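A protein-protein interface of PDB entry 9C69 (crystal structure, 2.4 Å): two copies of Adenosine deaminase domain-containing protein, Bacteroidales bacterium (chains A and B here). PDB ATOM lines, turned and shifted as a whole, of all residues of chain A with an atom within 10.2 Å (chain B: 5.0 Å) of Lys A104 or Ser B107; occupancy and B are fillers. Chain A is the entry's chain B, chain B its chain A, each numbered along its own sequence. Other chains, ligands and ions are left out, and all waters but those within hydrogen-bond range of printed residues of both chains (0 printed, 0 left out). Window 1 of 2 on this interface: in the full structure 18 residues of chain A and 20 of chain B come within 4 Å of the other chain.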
ATOM      1  N   SER A   8      -6.941  19.402 -13.405  1.00  0.00           N
ATOM      2  CA  SER A   8      -7.577  20.357 -14.290  1.00  0.00           C
ATOM      3  C   SER A   8      -7.084  21.739 -13.890  1.00  0.00           C
ATOM      4  O   SER A   8      -6.557  21.934 -12.796  1.00  0.00           O
ATOM      5  CB  SER A   8      -9.115  20.265 -14.221  1.00  0.00           C
ATOM      6  OG  SER A   8      -9.611  19.955 -12.897  1.00  0.00           O
ATOM      7  N   ALA A   9      -7.214  22.697 -14.794  1.00  0.00           N
ATOM      8  CA  ALA A   9      -6.791  24.058 -14.506  1.00  0.00           C
ATOM      9  C   ALA A   9      -7.880  25.039 -14.911  1.00  0.00           C
ATOM     10  O   ALA A   9      -8.587  24.831 -15.904  1.00  0.00           O
ATOM     11  CB  ALA A   9      -5.492  24.395 -15.239  1.00  0.00           C
ATOM     12  N   GLY A  10      -8.002  26.117 -14.146  1.00  0.00           N
ATOM     13  CA  GLY A  10      -8.905  27.182 -14.535  1.00  0.00           C
ATOM     14  C   GLY A  10      -8.252  28.549 -14.635  1.00  0.00           C
ATOM     15  O   GLY A  10      -7.108  28.670 -15.086  1.00  0.00           O
ATOM     16  N   THR A  35      -8.838  23.946 -21.023  1.00  0.00           N
ATOM     17  CA  THR A  35      -9.444  24.318 -22.291  1.00  0.00           C
ATOM     18  C   THR A  35      -8.507  25.225 -23.086  1.00  0.00           C
ATOM     19  O   THR A  35      -7.490  25.725 -22.588  1.00  0.00           O
ATOM     20  CB  THR A  35     -10.783  25.028 -22.085  1.00  0.00           C
ATOM     21  OG1 THR A  35     -10.598  26.167 -21.232  1.00  0.00           O
ATOM     22  CG2 THR A  35     -11.832  24.070 -21.495  1.00  0.00           C
ATOM     23  N   ILE A  68     -17.028  24.950 -22.495  1.00  0.00           N
ATOM     24  CA  ILE A  68     -18.035  23.906 -22.507  1.00  0.00           C
ATOM     25  C   ILE A  68     -19.378  24.620 -22.398  1.00  0.00           C
ATOM     26  O   ILE A  68     -19.789  25.039 -21.312  1.00  0.00           O
ATOM     27  CB  ILE A  68     -17.811  22.880 -21.393  1.00  0.00           C
ATOM     28  CG1 ILE A  68     -16.448  22.190 -21.606  1.00  0.00           C
ATOM     29  CG2 ILE A  68     -18.936  21.860 -21.386  1.00  0.00           C
ATOM     30  CD1 ILE A  68     -15.954  21.363 -20.421  1.00  0.00           C
ATOM     31  N   PHE A  74     -19.023  19.149 -23.913  1.00  0.00           N
ATOM     32  CA  PHE A  74     -18.608  18.366 -22.760  1.00  0.00           C
ATOM     33  C   PHE A  74     -18.064  17.024 -23.199  1.00  0.00           C
ATOM     34  O   PHE A  74     -17.037  16.555 -22.680  1.00  0.00           O
ATOM     35  CB  PHE A  74     -19.761  18.138 -21.786  1.00  0.00           C
ATOM     36  CG  PHE A  74     -19.395  17.204 -20.694  1.00  0.00           C
ATOM     37  CD1 PHE A  74     -18.555  17.634 -19.665  1.00  0.00           C
ATOM     38  CD2 PHE A  74     -19.802  15.875 -20.727  1.00  0.00           C
ATOM     39  CE1 PHE A  74     -18.162  16.761 -18.654  1.00  0.00           C
ATOM     40  CE2 PHE A  74     -19.425  14.993 -19.722  1.00  0.00           C
ATOM     41  CZ  PHE A  74     -18.592  15.435 -18.680  1.00  0.00           C
ATOM     42  N   TYR A  77     -14.614  17.352 -24.640  1.00  0.00           N
ATOM     43  CA  TYR A  77     -13.703  17.551 -23.527  1.00  0.00           C
ATOM     44  C   TYR A  77     -13.405  16.230 -22.830  1.00  0.00           C
ATOM     45  O   TYR A  77     -12.245  15.897 -22.572  1.00  0.00           O
ATOM     46  CB  TYR A  77     -14.290  18.555 -22.525  1.00  0.00           C
ATOM     47  CG  TYR A  77     -13.399  18.749 -21.312  1.00  0.00           C
ATOM     48  CD1 TYR A  77     -12.395  19.707 -21.319  1.00  0.00           C
ATOM     49  CD2 TYR A  77     -13.534  17.946 -20.172  1.00  0.00           C
ATOM     50  CE1 TYR A  77     -11.571  19.889 -20.237  1.00  0.00           C
ATOM     51  CE2 TYR A  77     -12.689  18.115 -19.068  1.00  0.00           C
ATOM     52  CZ  TYR A  77     -11.717  19.088 -19.117  1.00  0.00           C
ATOM     53  OH  TYR A  77     -10.885  19.285 -18.035  1.00  0.00           O
ATOM     54  N   GLN A  78     -14.451  15.463 -22.522  1.00  0.00           N
ATOM     55  CA  GLN A  78     -14.278  14.247 -21.736  1.00  0.00           C
ATOM     56  C   GLN A  78     -13.460  13.207 -22.491  1.00  0.00           C
ATOM     57  O   GLN A  78     -12.653  12.489 -21.887  1.00  0.00           O
ATOM     58  CB  GLN A  78     -15.639  13.675 -21.359  1.00  0.00           C
ATOM     59  CG  GLN A  78     -15.603  12.297 -20.754  1.00  0.00           C
ATOM     60  CD  GLN A  78     -16.702  12.162 -19.723  1.00  0.00           C
ATOM     61  OE1 GLN A  78     -16.584  12.684 -18.623  1.00  0.00           O
ATOM     62  NE2 GLN A  78     -17.797  11.501 -20.092  1.00  0.00           N
ATOM     63  N   LEU A  81      -9.865  14.381 -22.291  1.00  0.00           N
ATOM     64  CA  LEU A  81      -9.377  14.271 -20.920  1.00  0.00           C
ATOM     65  C   LEU A  81      -9.030  12.833 -20.575  1.00  0.00           C
ATOM     66  O   LEU A  81      -7.973  12.570 -19.981  1.00  0.00           O
ATOM     67  CB  LEU A  81     -10.401  14.804 -19.925  1.00  0.00           C
ATOM     68  CG  LEU A  81      -9.928  14.642 -18.481  1.00  0.00           C
ATOM     69  CD1 LEU A  81      -8.784  15.654 -18.189  1.00  0.00           C
ATOM     70  CD2 LEU A  81     -11.097  14.802 -17.503  1.00  0.00           C
ATOM     71  N   LEU A  99      -8.752  17.806  -7.836  1.00  0.00           N
ATOM     72  CA  LEU A  99     -10.030  18.089  -8.489  1.00  0.00           C
ATOM     73  C   LEU A  99     -10.403  19.569  -8.505  1.00  0.00           C
ATOM     74  O   LEU A  99     -11.440  19.926  -9.073  1.00  0.00           O
ATOM     75  CB  LEU A  99     -11.163  17.340  -7.774  1.00  0.00           C
ATOM     76  CG  LEU A  99     -11.258  15.827  -7.911  1.00  0.00           C
ATOM     77  CD1 LEU A  99     -12.555  15.360  -7.202  1.00  0.00           C
ATOM     78  CD2 LEU A  99     -11.207  15.408  -9.394  1.00  0.00           C
ATOM     79  N   SER A 100      -9.628  20.423  -7.848  1.00  0.00           N
ATOM     80  CA  SER A 100     -10.122  21.755  -7.539  1.00  0.00           C
ATOM     81  C   SER A 100     -10.130  22.687  -8.740  1.00  0.00           C
ATOM     82  O   SER A 100     -10.899  23.648  -8.746  1.00  0.00           O
ATOM     83  CB  SER A 100      -9.303  22.350  -6.399  1.00  0.00           C
ATOM     84  OG  SER A 100      -9.427  21.504  -5.261  1.00  0.00           O
ATOM     85  N   GLY A 101      -9.305  22.443  -9.754  1.00  0.00           N
ATOM     86  CA  GLY A 101      -9.232  23.380 -10.866  1.00  0.00           C
ATOM     87  C   GLY A 101     -10.369  23.207 -11.862  1.00  0.00           C
ATOM     88  O   GLY A 101     -10.991  22.153 -11.934  1.00  0.00           O
ATOM     89  N   GLY A 102     -10.663  24.289 -12.612  1.00  0.00           N
ATOM     90  CA  GLY A 102     -11.574  24.245 -13.749  1.00  0.00           C
ATOM     91  C   GLY A 102     -13.037  24.415 -13.371  1.00  0.00           C
ATOM     92  O   GLY A 102     -13.394  24.647 -12.215  1.00  0.00           O
ATOM     93  N   ILE A 103     -13.924  24.279 -14.366  1.00  0.00           N
ATOM     94  CA  ILE A 103     -15.348  24.374 -14.039  1.00  0.00           C
ATOM     95  C   ILE A 103     -15.801  23.036 -13.475  1.00  0.00           C
ATOM     96  O   ILE A 103     -15.083  22.031 -13.558  1.00  0.00           O
ATOM     97  CB  ILE A 103     -16.238  24.799 -15.228  1.00  0.00           C
ATOM     98  CG1 ILE A 103     -16.445  23.668 -16.217  1.00  0.00           C
ATOM     99  CG2 ILE A 103     -15.630  25.972 -15.991  1.00  0.00           C
ATOM    100  CD1 ILE A 103     -16.996  24.167 -17.532  1.00  0.00           C
ATOM    101  N   LYS A 104     -16.991  23.027 -12.886  1.00  0.00           N
ATOM    102  CA  LYS A 104     -17.470  21.838 -12.196  1.00  0.00           C
ATOM    103  C   LYS A 104     -17.525  20.629 -13.123  1.00  0.00           C
ATOM    104  O   LYS A 104     -17.121  19.527 -12.733  1.00  0.00           O
ATOM    105  CB  LYS A 104     -18.844  22.124 -11.586  1.00  0.00           C
ATOM    106  CG  LYS A 104     -18.802  22.995 -10.324  1.00  0.00           C
ATOM    107  CD  LYS A 104     -20.129  22.937  -9.603  1.00  0.00           C
ATOM    108  CE  LYS A 104     -20.116  23.669  -8.265  1.00  0.00           C
ATOM    109  NZ  LYS A 104     -20.146  25.139  -8.467  1.00  0.00           N
ATOM    110  N   SER A 105     -18.027  20.805 -14.353  1.00  0.00           N
ATOM    111  CA  SER A 105     -18.125  19.647 -15.234  1.00  0.00           C
ATOM    112  C   SER A 105     -16.740  19.114 -15.598  1.00  0.00           C
ATOM    113  O   SER A 105     -16.558  17.895 -15.684  1.00  0.00           O
ATOM    114  CB  SER A 105     -18.947  19.970 -16.487  1.00  0.00           C
ATOM    115  OG  SER A 105     -18.396  21.031 -17.232  1.00  0.00           O
ATOM    116  N   MET A 106     -15.744  19.995 -15.788  1.00  0.00           N
ATOM    117  CA  MET A 106     -14.380  19.498 -16.003  1.00  0.00           C
ATOM    118  C   MET A 106     -13.923  18.636 -14.832  1.00  0.00           C
ATOM    119  O   MET A 106     -13.381  17.536 -15.020  1.00  0.00           O
ATOM    120  CB  MET A 106     -13.385  20.641 -16.215  1.00  0.00           C
ATOM    121  CG  MET A 106     -13.516  21.413 -17.520  1.00  0.00           C
ATOM    122  SD  MET A 106     -12.761  23.067 -17.519  1.00  0.00           S
ATOM    123  CE  MET A 106     -11.091  22.666 -18.038  1.00  0.00           C
ATOM    124  N   SER A 107     -14.180  19.104 -13.613  1.00  0.00           N
ATOM    125  CA  SER A 107     -13.727  18.395 -12.429  1.00  0.00           C
ATOM    126  C   SER A 107     -14.467  17.059 -12.265  1.00  0.00           C
ATOM    127  O   SER A 107     -13.861  16.059 -11.855  1.00  0.00           O
ATOM    128  CB  SER A 107     -13.905  19.306 -11.208  1.00  0.00           C
ATOM    129  OG  SER A 107     -13.700  18.598  -9.992  1.00  0.00           O
ATOM    130  N   ALA A 108     -15.775  17.019 -12.565  1.00  0.00           N
ATOM    131  CA  ALA A 108     -16.511  15.763 -12.437  1.00  0.00           C
ATOM    132  C   ALA A 108     -16.002  14.721 -13.434  1.00  0.00           C
ATOM    133  O   ALA A 108     -15.942  13.525 -13.125  1.00  0.00           O
ATOM    134  CB  ALA A 108     -18.016  15.991 -12.641  1.00  0.00           C
ATOM    135  N   SER A 109     -15.665  15.155 -14.638  1.00  0.00           N
ATOM    136  CA  SER A 109     -15.132  14.236 -15.626  1.00  0.00           C
ATOM    137  C   SER A 109     -13.767  13.711 -15.187  1.00  0.00           C
ATOM    138  O   SER A 109     -13.452  12.528 -15.385  1.00  0.00           O
ATOM    139  CB  SER A 109     -15.069  14.940 -16.989  1.00  0.00           C
ATOM    140  OG  SER A 109     -14.516  14.094 -17.989  1.00  0.00           O
ATOM    141  N   LEU A 110     -12.956  14.561 -14.546  1.00  0.00           N
ATOM    142  CA  LEU A 110     -11.677  14.093 -14.028  1.00  0.00           C
ATOM    143  C   LEU A 110     -11.881  13.039 -12.936  1.00  0.00           C
ATOM    144  O   LEU A 110     -11.232  11.985 -12.950  1.00  0.00           O
ATOM    145  CB  LEU A 110     -10.855  15.282 -13.526  1.00  0.00           C
ATOM    146  CG  LEU A 110      -9.454  15.037 -12.937  1.00  0.00           C
ATOM    147  CD1 LEU A 110      -8.610  14.126 -13.816  1.00  0.00           C
ATOM    148  CD2 LEU A 110      -8.727  16.383 -12.691  1.00  0.00           C
ATOM    149  N   GLN A 111     -12.819  13.285 -12.002  1.00  0.00           N
ATOM    150  CA  GLN A 111     -13.098  12.295 -10.956  1.00  0.00           C
ATOM    151  C   GLN A 111     -13.600  10.974 -11.554  1.00  0.00           C
ATOM    152  O   GLN A 111     -13.257   9.876 -11.073  1.00  0.00           O
ATOM    153  CB  GLN A 111     -14.109  12.876  -9.957  1.00  0.00           C
ATOM    154  CG  GLN A 111     -14.865  11.852  -9.118  1.00  0.00           C
ATOM    155  CD  GLN A 111     -14.066  11.423  -7.888  1.00  0.00           C
ATOM    156  OE1 GLN A 111     -14.014  12.134  -6.872  1.00  0.00           O
ATOM    157  NE2 GLN A 111     -13.448  10.250  -7.970  1.00  0.00           N
ATOM    158  N   LYS A 112     -14.423  11.052 -12.603  1.00  0.00           N
ATOM    159  CA  LYS A 112     -14.873   9.814 -13.223  1.00  0.00           C
ATOM    160  C   LYS A 112     -13.685   9.046 -13.790  1.00  0.00           C
ATOM    161  O   LYS A 112     -13.585   7.827 -13.621  1.00  0.00           O
ATOM    162  CB  LYS A 112     -15.913  10.117 -14.313  1.00  0.00           C
ATOM    163  CG  LYS A 112     -16.626   8.890 -14.915  1.00  0.00           C
ATOM    164  CD  LYS A 112     -17.311   8.052 -13.849  1.00  0.00           C
ATOM    165  CE  LYS A 112     -18.681   8.646 -13.523  1.00  0.00           C
ATOM    166  NZ  LYS A 112     -19.246   8.092 -12.254  1.00  0.00           N
ATOM    167  N   HIS A 124      -9.159  17.588  -3.024  1.00  0.00           N
ATOM    168  CA  HIS A 124      -9.363  19.007  -3.246  1.00  0.00           C
ATOM    169  C   HIS A 124      -8.342  19.794  -2.429  1.00  0.00           C
ATOM    170  O   HIS A 124      -7.893  19.359  -1.358  1.00  0.00           O
ATOM    171  CB  HIS A 124     -10.773  19.459  -2.834  1.00  0.00           C
ATOM    172  CG  HIS A 124     -11.834  19.164  -3.844  1.00  0.00           C
ATOM    173  ND1 HIS A 124     -11.949  19.863  -5.023  1.00  0.00           N
ATOM    174  CD2 HIS A 124     -12.836  18.251  -3.845  1.00  0.00           C
ATOM    175  CE1 HIS A 124     -12.981  19.396  -5.709  1.00  0.00           C
ATOM    176  NE2 HIS A 124     -13.531  18.411  -5.020  1.00  0.00           N
ATOM    177  N   MET A 151     -10.803  12.805  -1.123  1.00  0.00           N
ATOM    178  CA  MET A 151     -12.126  12.307  -1.497  1.00  0.00           C
ATOM    179  C   MET A 151     -12.173  10.786  -1.613  1.00  0.00           C
ATOM    180  O   MET A 151     -13.256  10.207  -1.520  1.00  0.00           O
ATOM    181  CB  MET A 151     -12.587  12.903  -2.835  1.00  0.00           C
ATOM    182  CG  MET A 151     -12.694  14.421  -2.898  1.00  0.00           C
ATOM    183  SD  MET A 151     -13.477  15.180  -1.463  1.00  0.00           S
ATOM    184  CE  MET A 151     -15.205  14.895  -1.893  1.00  0.00           C
ATOM    185  N   SER B   8     -27.969  22.970  -5.114  1.00  0.00           N
ATOM    186  CA  SER B   8     -27.058  23.535  -4.133  1.00  0.00           C
ATOM    187  C   SER B   8     -26.894  25.020  -4.435  1.00  0.00           C
ATOM    188  O   SER B   8     -27.215  25.490  -5.529  1.00  0.00           O
ATOM    189  CB  SER B   8     -25.705  22.814  -4.153  1.00  0.00           C
ATOM    190  OG  SER B   8     -25.333  22.417  -5.481  1.00  0.00           O
ATOM    191  N   LEU B  99     -26.492  21.378 -10.743  1.00  0.00           N
ATOM    192  CA  LEU B  99     -25.248  21.106 -10.048  1.00  0.00           C
ATOM    193  C   LEU B  99     -24.389  22.351  -9.909  1.00  0.00           C
ATOM    194  O   LEU B  99     -23.291  22.288  -9.337  1.00  0.00           O
ATOM    195  CB  LEU B  99     -24.457  20.012 -10.797  1.00  0.00           C
ATOM    196  CG  LEU B  99     -24.976  18.570 -11.010  1.00  0.00           C
ATOM    197  CD1 LEU B  99     -23.950  17.723 -11.812  1.00  0.00           C
ATOM    198  CD2 LEU B  99     -25.325  17.866  -9.674  1.00  0.00           C
ATOM    199  N   SER B 100     -24.833  23.473 -10.446  1.00  0.00           N
ATOM    200  CA  SER B 100     -23.901  24.570 -10.621  1.00  0.00           C
ATOM    201  C   SER B 100     -23.607  25.327  -9.330  1.00  0.00           C
ATOM    202  O   SER B 100     -22.591  26.016  -9.263  1.00  0.00           O
ATOM    203  CB  SER B 100     -24.428  25.520 -11.694  1.00  0.00           C
ATOM    204  OG  SER B 100     -24.471  24.837 -12.929  1.00  0.00           O
ATOM    205  N   GLY B 101     -24.446  25.213  -8.311  1.00  0.00           N
ATOM    206  CA  GLY B 101     -24.248  25.972  -7.090  1.00  0.00           C
ATOM    207  C   GLY B 101     -23.349  25.266  -6.087  1.00  0.00           C
ATOM    208  O   GLY B 101     -23.272  24.044  -6.053  1.00  0.00           O
ATOM    209  N   GLY B 102     -22.665  26.070  -5.263  1.00  0.00           N
ATOM    210  CA  GLY B 102     -21.848  25.556  -4.180  1.00  0.00           C
ATOM    211  C   GLY B 102     -20.431  25.249  -4.624  1.00  0.00           C
ATOM    212  O   GLY B 102     -20.003  25.566  -5.743  1.00  0.00           O
ATOM    213  N   ILE B 103     -19.681  24.625  -3.722  1.00  0.00           N
ATOM    214  CA  ILE B 103     -18.311  24.264  -4.044  1.00  0.00           C
ATOM    215  C   ILE B 103     -18.318  22.906  -4.745  1.00  0.00           C
ATOM    216  O   ILE B 103     -19.301  22.154  -4.689  1.00  0.00           O
ATOM    217  CB  ILE B 103     -17.409  24.268  -2.790  1.00  0.00           C
ATOM    218  CG1 ILE B 103     -17.696  23.089  -1.893  1.00  0.00           C
ATOM    219  CG2 ILE B 103     -17.662  25.471  -1.923  1.00  0.00           C
ATOM    220  CD1 ILE B 103     -16.438  22.511  -1.378  1.00  0.00           C
ATOM    221  N   LYS B 104     -17.213  22.596  -5.429  1.00  0.00           N
ATOM    222  CA  LYS B 104     -17.165  21.398  -6.277  1.00  0.00           C
ATOM    223  C   LYS B 104     -17.602  20.151  -5.533  1.00  0.00           C
ATOM    224  O   LYS B 104     -18.337  19.318  -6.079  1.00  0.00           O
ATOM    225  CB  LYS B 104     -15.761  21.199  -6.839  1.00  0.00           C
ATOM    226  CG  LYS B 104     -15.477  22.233  -7.853  1.00  0.00           C
ATOM    227  CD  LYS B 104     -14.251  21.986  -8.697  1.00  0.00           C
ATOM    228  CE  LYS B 104     -13.868  23.360  -9.255  1.00  0.00           C
ATOM    229  NZ  LYS B 104     -12.903  23.245 -10.297  1.00  0.00           N
ATOM    230  N   SER B 105     -17.195  20.020  -4.273  1.00  0.00           N
ATOM    231  CA  SER B 105     -17.484  18.789  -3.567  1.00  0.00           C
ATOM    232  C   SER B 105     -18.936  18.728  -3.119  1.00  0.00           C
ATOM    233  O   SER B 105     -19.482  17.628  -2.987  1.00  0.00           O
ATOM    234  CB  SER B 105     -16.532  18.623  -2.370  1.00  0.00           C
ATOM    235  OG  SER B 105     -16.780  19.588  -1.354  1.00  0.00           O
ATOM    236  N   MET B 106     -19.558  19.881  -2.845  1.00  0.00           N
ATOM    237  CA  MET B 106     -21.000  19.914  -2.615  1.00  0.00           C
ATOM    238  C   MET B 106     -21.729  19.424  -3.855  1.00  0.00           C
ATOM    239  O   MET B 106     -22.607  18.558  -3.784  1.00  0.00           O
ATOM    240  CB  MET B 106     -21.445  21.337  -2.276  1.00  0.00           C
ATOM    241  CG  MET B 106     -20.992  21.847  -0.920  1.00  0.00           C
ATOM    242  SD  MET B 106     -21.303  23.627  -0.733  1.00  0.00           S
ATOM    243  CE  MET B 106     -23.098  23.666  -0.578  1.00  0.00           C
ATOM    244  N   SER B 107     -21.324  19.943  -5.013  1.00  0.00           N
ATOM    245  CA  SER B 107     -21.968  19.597  -6.271  1.00  0.00           C
ATOM    246  C   SER B 107     -21.753  18.127  -6.620  1.00  0.00           C
ATOM    247  O   SER B 107     -22.692  17.444  -7.060  1.00  0.00           O
ATOM    248  CB  SER B 107     -21.441  20.515  -7.375  1.00  0.00           C
ATOM    249  OG  SER B 107     -21.833  20.090  -8.665  1.00  0.00           O
ATOM    250  N   ALA B 108     -20.532  17.621  -6.423  1.00  0.00           N
ATOM    251  CA  ALA B 108     -20.279  16.213  -6.716  1.00  0.00           C
ATOM    252  C   ALA B 108     -21.068  15.312  -5.783  1.00  0.00           C
ATOM    253  O   ALA B 108     -21.482  14.222  -6.184  1.00  0.00           O
ATOM    254  CB  ALA B 108     -18.786  15.887  -6.616  1.00  0.00           C
ATOM    255  N   SER B 109     -21.304  15.749  -4.551  1.00  0.00           N
ATOM    256  CA  SER B 109     -22.115  14.921  -3.670  1.00  0.00           C
ATOM    257  C   SER B 109     -23.560  14.900  -4.136  1.00  0.00           C
ATOM    258  O   SER B 109     -24.259  13.892  -3.961  1.00  0.00           O
ATOM    259  CB  SER B 109     -22.016  15.418  -2.226  1.00  0.00           C
ATOM    260  OG  SER B 109     -22.857  14.654  -1.383  1.00  0.00           O
ATOM    261  N   LEU B 110     -24.019  15.997  -4.747  1.00  0.00           N
ATOM    262  CA  LEU B 110     -25.391  16.044  -5.232  1.00  0.00           C
ATOM    263  C   LEU B 110     -25.537  15.182  -6.483  1.00  0.00           C
ATOM    264  O   LEU B 110     -26.516  14.443  -6.619  1.00  0.00           O
ATOM    265  CB  LEU B 110     -25.801  17.509  -5.469  1.00  0.00           C
ATOM    266  CG  LEU B 110     -27.192  17.847  -6.023  1.00  0.00           C
ATOM    267  CD1 LEU B 110     -28.279  17.190  -5.200  1.00  0.00           C
ATOM    268  CD2 LEU B 110     -27.411  19.384  -6.123  1.00  0.00           C
ATOM    269  N   GLN B 111     -24.547  15.231  -7.382  1.00  0.00           N
ATOM    270  CA  GLN B 111     -24.524  14.318  -8.524  1.00  0.00           C
ATOM    271  C   GLN B 111     -24.600  12.863  -8.074  1.00  0.00           C
ATOM    272  O   GLN B 111     -25.358  12.065  -8.653  1.00  0.00           O
ATOM    273  CB  GLN B 111     -23.264  14.543  -9.376  1.00  0.00           C
ATOM    274  CG  GLN B 111     -22.969  13.407 -10.380  1.00  0.00           C
ATOM    275  CD  GLN B 111     -23.906  13.455 -11.597  1.00  0.00           C
ATOM    276  OE1 GLN B 111     -23.681  14.200 -12.561  1.00  0.00           O
ATOM    277  NE2 GLN B 111     -24.943  12.630 -11.570  1.00  0.00           N
ATOM    278  N   HIS B 124     -26.137  21.567 -15.594  1.00  0.00           N
ATOM    279  CA  HIS B 124     -25.425  22.793 -15.261  1.00  0.00           C
ATOM    280  C   HIS B 124     -26.090  23.968 -15.957  1.00  0.00           C
ATOM    281  O   HIS B 124     -26.653  23.826 -17.045  1.00  0.00           O
ATOM    282  CB  HIS B 124     -23.954  22.731 -15.695  1.00  0.00           C
ATOM    283  CG  HIS B 124     -23.108  21.878 -14.811  1.00  0.00           C
ATOM    284  ND1 HIS B 124     -22.827  22.217 -13.505  1.00  0.00           N
ATOM    285  CD2 HIS B 124     -22.506  20.686 -15.032  1.00  0.00           C
ATOM    286  CE1 HIS B 124     -22.067  21.281 -12.964  1.00  0.00           C
ATOM    287  NE2 HIS B 124     -21.860  20.340 -13.869  1.00  0.00           N
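The side-chain amino group of Lys A104 is in hydrogen-bond range of the backbone carbonyl oxygen of Ser B100 (2.7 Å).
The backbone carbonyl oxygen of Gly B102 lies within hydrogen-bond range of the side-chain amino group of Lys A104 (2.8 Å).
The backbone carbonyl oxygen (O) of Ser A100 is in hydrogen-bond range of the side-chain amino group (NZ) of Lys B104 (2.6 Å).
The side-chain amino group of Lys B104 is in hydrogen-bond range of the backbone carbonyl oxygen of Gly A101 (2.7 Å).
The backbone carbonyl oxygen of Gly A102 sits at hydrogen-bond distance from the side-chain amino group of Lys B104.
The side-chain hydroxyl (OG) of Ser B107 sits at hydrogen-bond distance from the backbone carbonyl oxygen (O) of Leu B99, 2.7 Å away.
OG of Ser B100 lies within hydrogen-bond range of ND1 of His B124, 3.1 Å away.
The backbone NH (N) of Ile B103 sits at hydrogen-bond distance from the side-chain sulfur (SD) of Met B106 (3.5 Å).
The backbone carbonyl oxygen (O) of Gly A101 is in hydrogen-bond range of the side-chain hydroxyl (OG) of Ser A8 (2.8 Å).
The backbone carbonyl oxygen (O) of Leu A99 sits at hydrogen-bond distance from the side-chain hydroxyl (OG) of Ser A107 (2.8 Å).
The side-chain hydroxyl (OG) of Ser A100 lies within hydrogen-bond range of a ring nitrogen (ND1) of His A124 (3.0 Å).
Lys B104 touches Leu A99 (CD to O, 3.5 Å).
CD of Lys A104 touches O of Leu B99 (3.2 Å).
O of Gly B101 touches CE of Lys A104, 3.9 Å away.
CE of Lys A104 touches O of Ile B103, at 3.97 Å.
CD of Lys A104 touches OG of Ser B107, 3.4 Å away.
His B124 touches Lys A104 (CE1 to CB, 3.6 Å).
NE2 of His B124 touches N of Ser A105, at 3.9 Å.
Ser A107 touches Lys B104.
His A124 touches Lys B104.
CB of Ser B105 touches CD2 of His A124, at 3.997 Å.
Lys A104 touches seven residues of chain B.
Ser B107 touches one residue of chain A.
Leu B99 touches just one residue of chain A: Lys A104.
Ser B100 touches just one residue of chain A: Lys A104 (2.7 Å).
Gly B101 touches just one residue of chain A: Lys A104.
Of chain A, only Leu A99, Ser A100, Gly A101, Gly A102, Ser A107 and His A124 come within 4 Å of Lys B104.
No residue of chain A comes within 4 Å of Ala B108.
No residue of chain A comes within 4 Å of Leu B110.
Of the printed residues of chain B, Met A151 touches Ser B105 (3.99 Å).
Printed residues of chain A within 4 Å of His B124: Lys A104 and Ser A105.
Of the printed residues of chain B, Gly A101 touches Lys B104 (2.7 Å).
Tyr A77 touches none of the printed residues of chain B.
Gln A78 touches none of the printed residues of chain B.
The nearest residue of chain B that does not touch Lys A104 is Lys B104 (4.2 Å).
The nearest printed residue of chain A that does not touch Ser B107 is Ala A108 (6.9 Å).
The nearest printed residue of chain A that does not touch Ser B105 is Lys A104 (6.1 Å).
Hydrophobic or aromatic side chains of chain B that line the printed part of chain A: His B124.
Among the printed residues, 16 pairs touch across the chains.
Among the printed residues, no Asp or Glu carboxylate lies within 4 Å of a Lys or Arg side-chain nitrogen of the other chain.
Ser A100 touches Lys B104, and with the chains exchanged Lys A104 touches Ser B100.
Gly A101 touches Lys B104, and with the chains exchanged Lys A104 touches Gly B101.
Lys A104 touches Ser B107, and with the chains exchanged Ser A107 touches Lys B104.
Lys A104 touches His B124, and with the chains exchanged His A124 touches Lys B104.
Positions printed for both chains: 8, 99, 100, 101, 102, 103, 104, 105, 106, 107, 108, 109, 110, 111 and 124.
Of the 16 pairs that touch across the chains among the printed residues, 14 have their exchanged pair printed and touching as well.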
